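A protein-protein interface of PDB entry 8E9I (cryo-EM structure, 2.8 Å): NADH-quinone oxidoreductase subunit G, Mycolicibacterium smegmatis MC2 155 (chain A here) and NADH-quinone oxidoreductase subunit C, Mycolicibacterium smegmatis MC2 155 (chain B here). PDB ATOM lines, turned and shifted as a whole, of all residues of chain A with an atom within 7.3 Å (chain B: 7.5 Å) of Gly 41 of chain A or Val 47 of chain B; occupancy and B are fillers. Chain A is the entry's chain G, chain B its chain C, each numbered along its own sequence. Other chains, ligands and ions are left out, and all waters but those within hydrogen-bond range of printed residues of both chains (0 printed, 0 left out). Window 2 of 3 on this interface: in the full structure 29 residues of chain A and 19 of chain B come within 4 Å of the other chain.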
ATOM      1  N   ARG A  35      18.428  10.350   2.876  1.00  0.00           N
ATOM      2  CA  ARG A  35      19.113  10.556   4.147  1.00  0.00           C
ATOM      3  C   ARG A  35      19.305   9.244   4.889  1.00  0.00           C
ATOM      4  O   ARG A  35      20.377   8.989   5.445  1.00  0.00           O
ATOM      5  CB  ARG A  35      18.337  11.543   5.011  1.00  0.00           C
ATOM      6  CG  ARG A  35      18.115  12.869   4.344  1.00  0.00           C
ATOM      7  CD  ARG A  35      19.396  13.646   4.243  1.00  0.00           C
ATOM      8  NE  ARG A  35      19.324  14.634   3.179  1.00  0.00           N
ATOM      9  CZ  ARG A  35      19.969  14.552   2.025  1.00  0.00           C
ATOM     10  NH1 ARG A  35      20.757  13.529   1.741  1.00  0.00           N
ATOM     11  NH2 ARG A  35      19.821  15.520   1.132  1.00  0.00           N
ATOM     12  N   ALA A  36      18.277   8.400   4.918  1.00  0.00           N
ATOM     13  CA  ALA A  36      18.411   7.113   5.584  1.00  0.00           C
ATOM     14  C   ALA A  36      19.497   6.275   4.924  1.00  0.00           C
ATOM     15  O   ALA A  36      20.348   5.690   5.603  1.00  0.00           O
ATOM     16  CB  ALA A  36      17.070   6.381   5.563  1.00  0.00           C
ATOM     17  N   ALA A  37      19.491   6.217   3.593  1.00  0.00           N
ATOM     18  CA  ALA A  37      20.493   5.423   2.894  1.00  0.00           C
ATOM     19  C   ALA A  37      21.887   5.985   3.120  1.00  0.00           C
ATOM     20  O   ALA A  37      22.872   5.237   3.126  1.00  0.00           O
ATOM     21  CB  ALA A  37      20.172   5.365   1.403  1.00  0.00           C
ATOM     22  N   GLU A  38      21.999   7.302   3.284  1.00  0.00           N
ATOM     23  CA  GLU A  38      23.268   7.871   3.714  1.00  0.00           C
ATOM     24  C   GLU A  38      23.651   7.335   5.081  1.00  0.00           C
ATOM     25  O   GLU A  38      24.778   6.873   5.288  1.00  0.00           O
ATOM     26  CB  GLU A  38      23.176   9.396   3.750  1.00  0.00           C
ATOM     27  CG  GLU A  38      23.159  10.057   2.384  1.00  0.00           C
ATOM     28  CD  GLU A  38      23.076  11.568   2.468  1.00  0.00           C
ATOM     29  OE1 GLU A  38      22.073  12.085   2.997  1.00  0.00           O
ATOM     30  OE2 GLU A  38      24.001  12.244   1.980  1.00  0.00           O
ATOM     31  N   LEU A  39      22.710   7.364   6.021  1.00  0.00           N
ATOM     32  CA  LEU A  39      23.007   6.945   7.384  1.00  0.00           C
ATOM     33  C   LEU A  39      23.431   5.489   7.447  1.00  0.00           C
ATOM     34  O   LEU A  39      24.219   5.118   8.321  1.00  0.00           O
ATOM     35  CB  LEU A  39      21.791   7.169   8.275  1.00  0.00           C
ATOM     36  CG  LEU A  39      21.415   8.628   8.501  1.00  0.00           C
ATOM     37  CD1 LEU A  39      20.096   8.721   9.246  1.00  0.00           C
ATOM     38  CD2 LEU A  39      22.518   9.327   9.264  1.00  0.00           C
ATOM     39  N   MET A  40      22.930   4.652   6.546  1.00  0.00           N
ATOM     40  CA  MET A  40      23.272   3.240   6.611  1.00  0.00           C
ATOM     41  C   MET A  40      24.456   2.887   5.717  1.00  0.00           C
ATOM     42  O   MET A  40      24.865   1.725   5.687  1.00  0.00           O
ATOM     43  CB  MET A  40      22.040   2.393   6.263  1.00  0.00           C
ATOM     44  CG  MET A  40      22.257   0.897   6.368  1.00  0.00           C
ATOM     45  SD  MET A  40      20.796  -0.081   6.000  1.00  0.00           S
ATOM     46  CE  MET A  40      20.643   0.105   4.238  1.00  0.00           C
ATOM     47  N   GLY A  41      25.040   3.861   5.024  1.00  0.00           N
ATOM     48  CA  GLY A  41      26.263   3.641   4.278  1.00  0.00           C
ATOM     49  C   GLY A  41      26.096   3.409   2.795  1.00  0.00           C
ATOM     50  O   GLY A  41      27.002   2.855   2.166  1.00  0.00           O
ATOM     51  N   ILE A  42      24.984   3.835   2.209  1.00  0.00           N
ATOM     52  CA  ILE A  42      24.651   3.521   0.828  1.00  0.00           C
ATOM     53  C   ILE A  42      24.623   4.807   0.026  1.00  0.00           C
ATOM     54  O   ILE A  42      23.900   5.751   0.364  1.00  0.00           O
ATOM     55  CB  ILE A  42      23.317   2.769   0.740  1.00  0.00           C
ATOM     56  CG1 ILE A  42      23.453   1.433   1.464  1.00  0.00           C
ATOM     57  CG2 ILE A  42      22.914   2.556  -0.698  1.00  0.00           C
ATOM     58  CD1 ILE A  42      23.134   1.505   2.910  1.00  0.00           C
ATOM     59  N   GLN A  43      25.415   4.840  -1.040  1.00  0.00           N
ATOM     60  CA  GLN A  43      25.580   6.028  -1.866  1.00  0.00           C
ATOM     61  C   GLN A  43      24.585   5.955  -3.010  1.00  0.00           C
ATOM     62  O   GLN A  43      24.869   5.413  -4.077  1.00  0.00           O
ATOM     63  CB  GLN A  43      27.008   6.125  -2.384  1.00  0.00           C
ATOM     64  CG  GLN A  43      27.251   7.304  -3.296  1.00  0.00           C
ATOM     65  CD  GLN A  43      28.723   7.548  -3.552  1.00  0.00           C
ATOM     66  OE1 GLN A  43      29.529   7.603  -2.624  1.00  0.00           O
ATOM     67  NE2 GLN A  43      29.082   7.711  -4.821  1.00  0.00           N
ATOM     68  N   ILE A  44      23.402   6.501  -2.787  1.00  0.00           N
ATOM     69  CA  ILE A  44      22.450   6.669  -3.881  1.00  0.00           C
ATOM     70  C   ILE A  44      22.886   7.869  -4.716  1.00  0.00           C
ATOM     71  O   ILE A  44      23.077   8.958  -4.158  1.00  0.00           O
ATOM     72  CB  ILE A  44      21.039   6.861  -3.341  1.00  0.00           C
ATOM     73  CG1 ILE A  44      20.621   5.646  -2.518  1.00  0.00           C
ATOM     74  CG2 ILE A  44      20.063   7.068  -4.479  1.00  0.00           C
ATOM     75  CD1 ILE A  44      19.366   5.855  -1.734  1.00  0.00           C
ATOM     76  N   PHE A  90      22.258  -1.044  -5.563  1.00  0.00           N
ATOM     77  CA  PHE A  90      23.113  -2.107  -5.065  1.00  0.00           C
ATOM     78  C   PHE A  90      22.393  -3.443  -5.001  1.00  0.00           C
ATOM     79  O   PHE A  90      23.053  -4.484  -4.967  1.00  0.00           O
ATOM     80  CB  PHE A  90      23.645  -1.735  -3.686  1.00  0.00           C
ATOM     81  CG  PHE A  90      24.677  -0.657  -3.718  1.00  0.00           C
ATOM     82  CD1 PHE A  90      25.920  -0.891  -4.276  1.00  0.00           C
ATOM     83  CD2 PHE A  90      24.408   0.594  -3.201  1.00  0.00           C
ATOM     84  CE1 PHE A  90      26.873   0.102  -4.311  1.00  0.00           C
ATOM     85  CE2 PHE A  90      25.357   1.588  -3.233  1.00  0.00           C
ATOM     86  CZ  PHE A  90      26.592   1.342  -3.787  1.00  0.00           C
ATOM     87  N   VAL B  27      36.297   5.272   8.810  1.00  0.00           N
ATOM     88  CA  VAL B  27      34.906   5.636   8.589  1.00  0.00           C
ATOM     89  C   VAL B  27      34.875   6.799   7.609  1.00  0.00           C
ATOM     90  O   VAL B  27      35.060   7.956   8.001  1.00  0.00           O
ATOM     91  CB  VAL B  27      34.199   5.993   9.903  1.00  0.00           C
ATOM     92  CG1 VAL B  27      32.789   6.478   9.635  1.00  0.00           C
ATOM     93  CG2 VAL B  27      34.186   4.785  10.820  1.00  0.00           C
ATOM     94  N   ARG B  28      34.635   6.489   6.338  1.00  0.00           N
ATOM     95  CA  ARG B  28      34.567   7.519   5.315  1.00  0.00           C
ATOM     96  C   ARG B  28      33.342   8.389   5.548  1.00  0.00           C
ATOM     97  O   ARG B  28      32.251   7.880   5.816  1.00  0.00           O
ATOM     98  CB  ARG B  28      34.500   6.879   3.929  1.00  0.00           C
ATOM     99  CG  ARG B  28      35.738   6.089   3.529  1.00  0.00           C
ATOM    100  CD  ARG B  28      36.830   6.986   2.985  1.00  0.00           C
ATOM    101  NE  ARG B  28      37.553   7.680   4.042  1.00  0.00           N
ATOM    102  CZ  ARG B  28      38.536   7.145   4.753  1.00  0.00           C
ATOM    103  NH1 ARG B  28      38.943   5.903   4.549  1.00  0.00           N
ATOM    104  NH2 ARG B  28      39.129   7.878   5.692  1.00  0.00           N
ATOM    105  N   ARG B  29      33.522   9.700   5.456  1.00  0.00           N
ATOM    106  CA  ARG B  29      32.431  10.651   5.593  1.00  0.00           C
ATOM    107  C   ARG B  29      32.217  11.365   4.269  1.00  0.00           C
ATOM    108  O   ARG B  29      33.145  11.956   3.715  1.00  0.00           O
ATOM    109  CB  ARG B  29      32.727  11.677   6.690  1.00  0.00           C
ATOM    110  CG  ARG B  29      32.599  11.142   8.105  1.00  0.00           C
ATOM    111  CD  ARG B  29      31.217  10.580   8.382  1.00  0.00           C
ATOM    112  NE  ARG B  29      30.151  11.467   7.926  1.00  0.00           N
ATOM    113  CZ  ARG B  29      29.459  12.284   8.710  1.00  0.00           C
ATOM    114  NH1 ARG B  29      29.688  12.358  10.012  1.00  0.00           N
ATOM    115  NH2 ARG B  29      28.512  13.046   8.174  1.00  0.00           N
ATOM    116  N   GLY B  30      30.991  11.308   3.763  1.00  0.00           N
ATOM    117  CA  GLY B  30      30.673  11.982   2.521  1.00  0.00           C
ATOM    118  C   GLY B  30      30.998  11.157   1.297  1.00  0.00           C
ATOM    119  O   GLY B  30      31.693  10.144   1.388  1.00  0.00           O
ATOM    120  N   MET B  31      30.499  11.583   0.142  1.00  0.00           N
ATOM    121  CA  MET B  31      30.762  10.862  -1.090  1.00  0.00           C
ATOM    122  C   MET B  31      32.106  11.284  -1.681  1.00  0.00           C
ATOM    123  O   MET B  31      32.722  12.269  -1.271  1.00  0.00           O
ATOM    124  CB  MET B  31      29.646  11.108  -2.101  1.00  0.00           C
ATOM    125  CG  MET B  31      28.382  10.331  -1.812  1.00  0.00           C
ATOM    126  SD  MET B  31      27.457  10.974  -0.418  1.00  0.00           S
ATOM    127  CE  MET B  31      26.764  12.439  -1.157  1.00  0.00           C
ATOM    128  N   GLY B  44      28.393  15.632   1.879  1.00  0.00           N
ATOM    129  CA  GLY B  44      29.209  15.117   2.956  1.00  0.00           C
ATOM    130  C   GLY B  44      28.489  14.341   4.028  1.00  0.00           C
ATOM    131  O   GLY B  44      29.104  13.991   5.038  1.00  0.00           O
ATOM    132  N   ARG B  45      27.205  14.052   3.855  1.00  0.00           N
ATOM    133  CA  ARG B  45      26.415  13.487   4.935  1.00  0.00           C
ATOM    134  C   ARG B  45      26.450  11.966   4.978  1.00  0.00           C
ATOM    135  O   ARG B  45      25.977  11.382   5.955  1.00  0.00           O
ATOM    136  CB  ARG B  45      24.966  13.964   4.820  1.00  0.00           C
ATOM    137  CG  ARG B  45      24.171  13.786   6.089  1.00  0.00           C
ATOM    138  CD  ARG B  45      22.891  14.585   6.050  1.00  0.00           C
ATOM    139  NE  ARG B  45      23.151  16.018   6.114  1.00  0.00           N
ATOM    140  CZ  ARG B  45      22.336  16.906   6.665  1.00  0.00           C
ATOM    141  NH1 ARG B  45      21.200  16.544   7.238  1.00  0.00           N
ATOM    142  NH2 ARG B  45      22.670  18.193   6.642  1.00  0.00           N
ATOM    143  N   LEU B  46      27.009  11.315   3.964  1.00  0.00           N
ATOM    144  CA  LEU B  46      27.114   9.863   3.984  1.00  0.00           C
ATOM    145  C   LEU B  46      28.079   9.424   5.076  1.00  0.00           C
ATOM    146  O   LEU B  46      29.059  10.111   5.367  1.00  0.00           O
ATOM    147  CB  LEU B  46      27.587   9.352   2.627  1.00  0.00           C
ATOM    148  CG  LEU B  46      27.851   7.852   2.522  1.00  0.00           C
ATOM    149  CD1 LEU B  46      26.559   7.091   2.627  1.00  0.00           C
ATOM    150  CD2 LEU B  46      28.546   7.521   1.223  1.00  0.00           C
ATOM    151  N   VAL B  47      27.798   8.274   5.680  1.00  0.00           N
ATOM    152  CA  VAL B  47      28.667   7.671   6.683  1.00  0.00           C
ATOM    153  C   VAL B  47      28.923   6.229   6.271  1.00  0.00           C
ATOM    154  O   VAL B  47      28.084   5.352   6.507  1.00  0.00           O
ATOM    155  CB  VAL B  47      28.049   7.731   8.087  1.00  0.00           C
ATOM    156  CG1 VAL B  47      28.956   7.051   9.084  1.00  0.00           C
ATOM    157  CG2 VAL B  47      27.793   9.160   8.497  1.00  0.00           C
ATOM    158  N   ARG B  48      30.085   5.980   5.673  1.00  0.00           N
ATOM    159  CA  ARG B  48      30.447   4.654   5.177  1.00  0.00           C
ATOM    160  C   ARG B  48      31.612   4.122   6.001  1.00  0.00           C
ATOM    161  O   ARG B  48      32.762   4.548   5.800  1.00  0.00           O
ATOM    162  CB  ARG B  48      30.813   4.703   3.700  1.00  0.00           C
ATOM    163  N   PRO B  49      31.364   3.213   6.943  1.00  0.00           N
ATOM    164  CA  PRO B  49      32.482   2.592   7.658  1.00  0.00           C
ATOM    165  C   PRO B  49      33.289   1.700   6.731  1.00  0.00           C
ATOM    166  O   PRO B  49      32.750   1.085   5.808  1.00  0.00           O
ATOM    167  CB  PRO B  49      31.792   1.787   8.763  1.00  0.00           C
ATOM    168  CG  PRO B  49      30.452   1.493   8.223  1.00  0.00           C
ATOM    169  CD  PRO B  49      30.068   2.661   7.371  1.00  0.00           C
ATOM    170  N   VAL B  50      34.594   1.636   6.984  1.00  0.00           N
ATOM    171  CA  VAL B  50      35.509   0.849   6.159  1.00  0.00           C
ATOM    172  C   VAL B  50      35.775  -0.443   6.922  1.00  0.00           C
ATOM    173  O   VAL B  50      36.686  -0.533   7.746  1.00  0.00           O
ATOM    174  CB  VAL B  50      36.794   1.607   5.844  1.00  0.00           C
ATOM    175  CG1 VAL B  50      37.676   0.780   4.935  1.00  0.00           C
ATOM    176  CG2 VAL B  50      36.479   2.944   5.214  1.00  0.00           C
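Of the 11 printed residues of chain A, 4 touch a printed residue of chain B. Of the 12 printed residues of chain B, 4 touch a printed residue of chain A. Printed residues of chain B that touch a printed residue of chain A: Met 31, Arg 45, Leu 46 and Val 47. Along chain B the printed residues that touch a printed residue of chain A span positions 31 to 47.
The backbone carbonyl oxygen (O) of Glu 38 of chain A sits at hydrogen-bond distance from the backbone NH (N) of Val 47 of chain B, at 3.4 Å.
Of chain B, only Leu 46 and Val 47 come within 4 Å of Gly 41 of chain A. Of chain A, only Glu 38 (3.4 Å) and Gly 41 (3.3 Å) come within 4 Å of Val 47 of chain B. Of the printed residues of chain A, Arg 45 of chain B touches Glu 38. Printed residues of chain B within 4 Å of Ile 42 of chain A: Leu 46. Printed residues of chain A within 4 Å of Met 31 of chain B: Gln 43. The nearest residue of chain A that does not touch Val 47 of chain B is Leu 39 of chain A (4.3 Å). The nearest printed residue of chain A that does not touch Arg 45 of chain B is Arg 35 of chain A (4.04 Å).
The backbone carbonyl oxygen (O) of Leu 46 of chain B is in hydrogen-bond range of the guanidinium group (NE) of Arg 29 of chain B, 3.1 Å away. The backbone NH of Gly 30 of chain B lies within hydrogen-bond range of the backbone carbonyl oxygen of Leu 46 of chain B. The guanidinium group (NH1) of Arg 35 of chain A is in salt-bridge range of the side-chain carboxylate (OE2) of Glu 38 of chain A (3.5 Å). The backbone carbonyl oxygen of Ala 37 of chain A lies within hydrogen-bond range of the backbone NH of Ile 42 of chain A, at 2.7 Å.
Among the printed residues, pairs that only touch across the chains: Glu 38 of chain A with Arg 45 of chain B, Glu 38 of chain A with Leu 46 of chain B, Gly 41 of chain A with Leu 46 of chain B, Gly 41 of chain A with Val 47 of chain B, Ile 42 of chain A with Leu 46 of chain B, Gln 43 of chain A with Met 31 of chain B and Gln 43 of chain A with Leu 46 of chain B.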
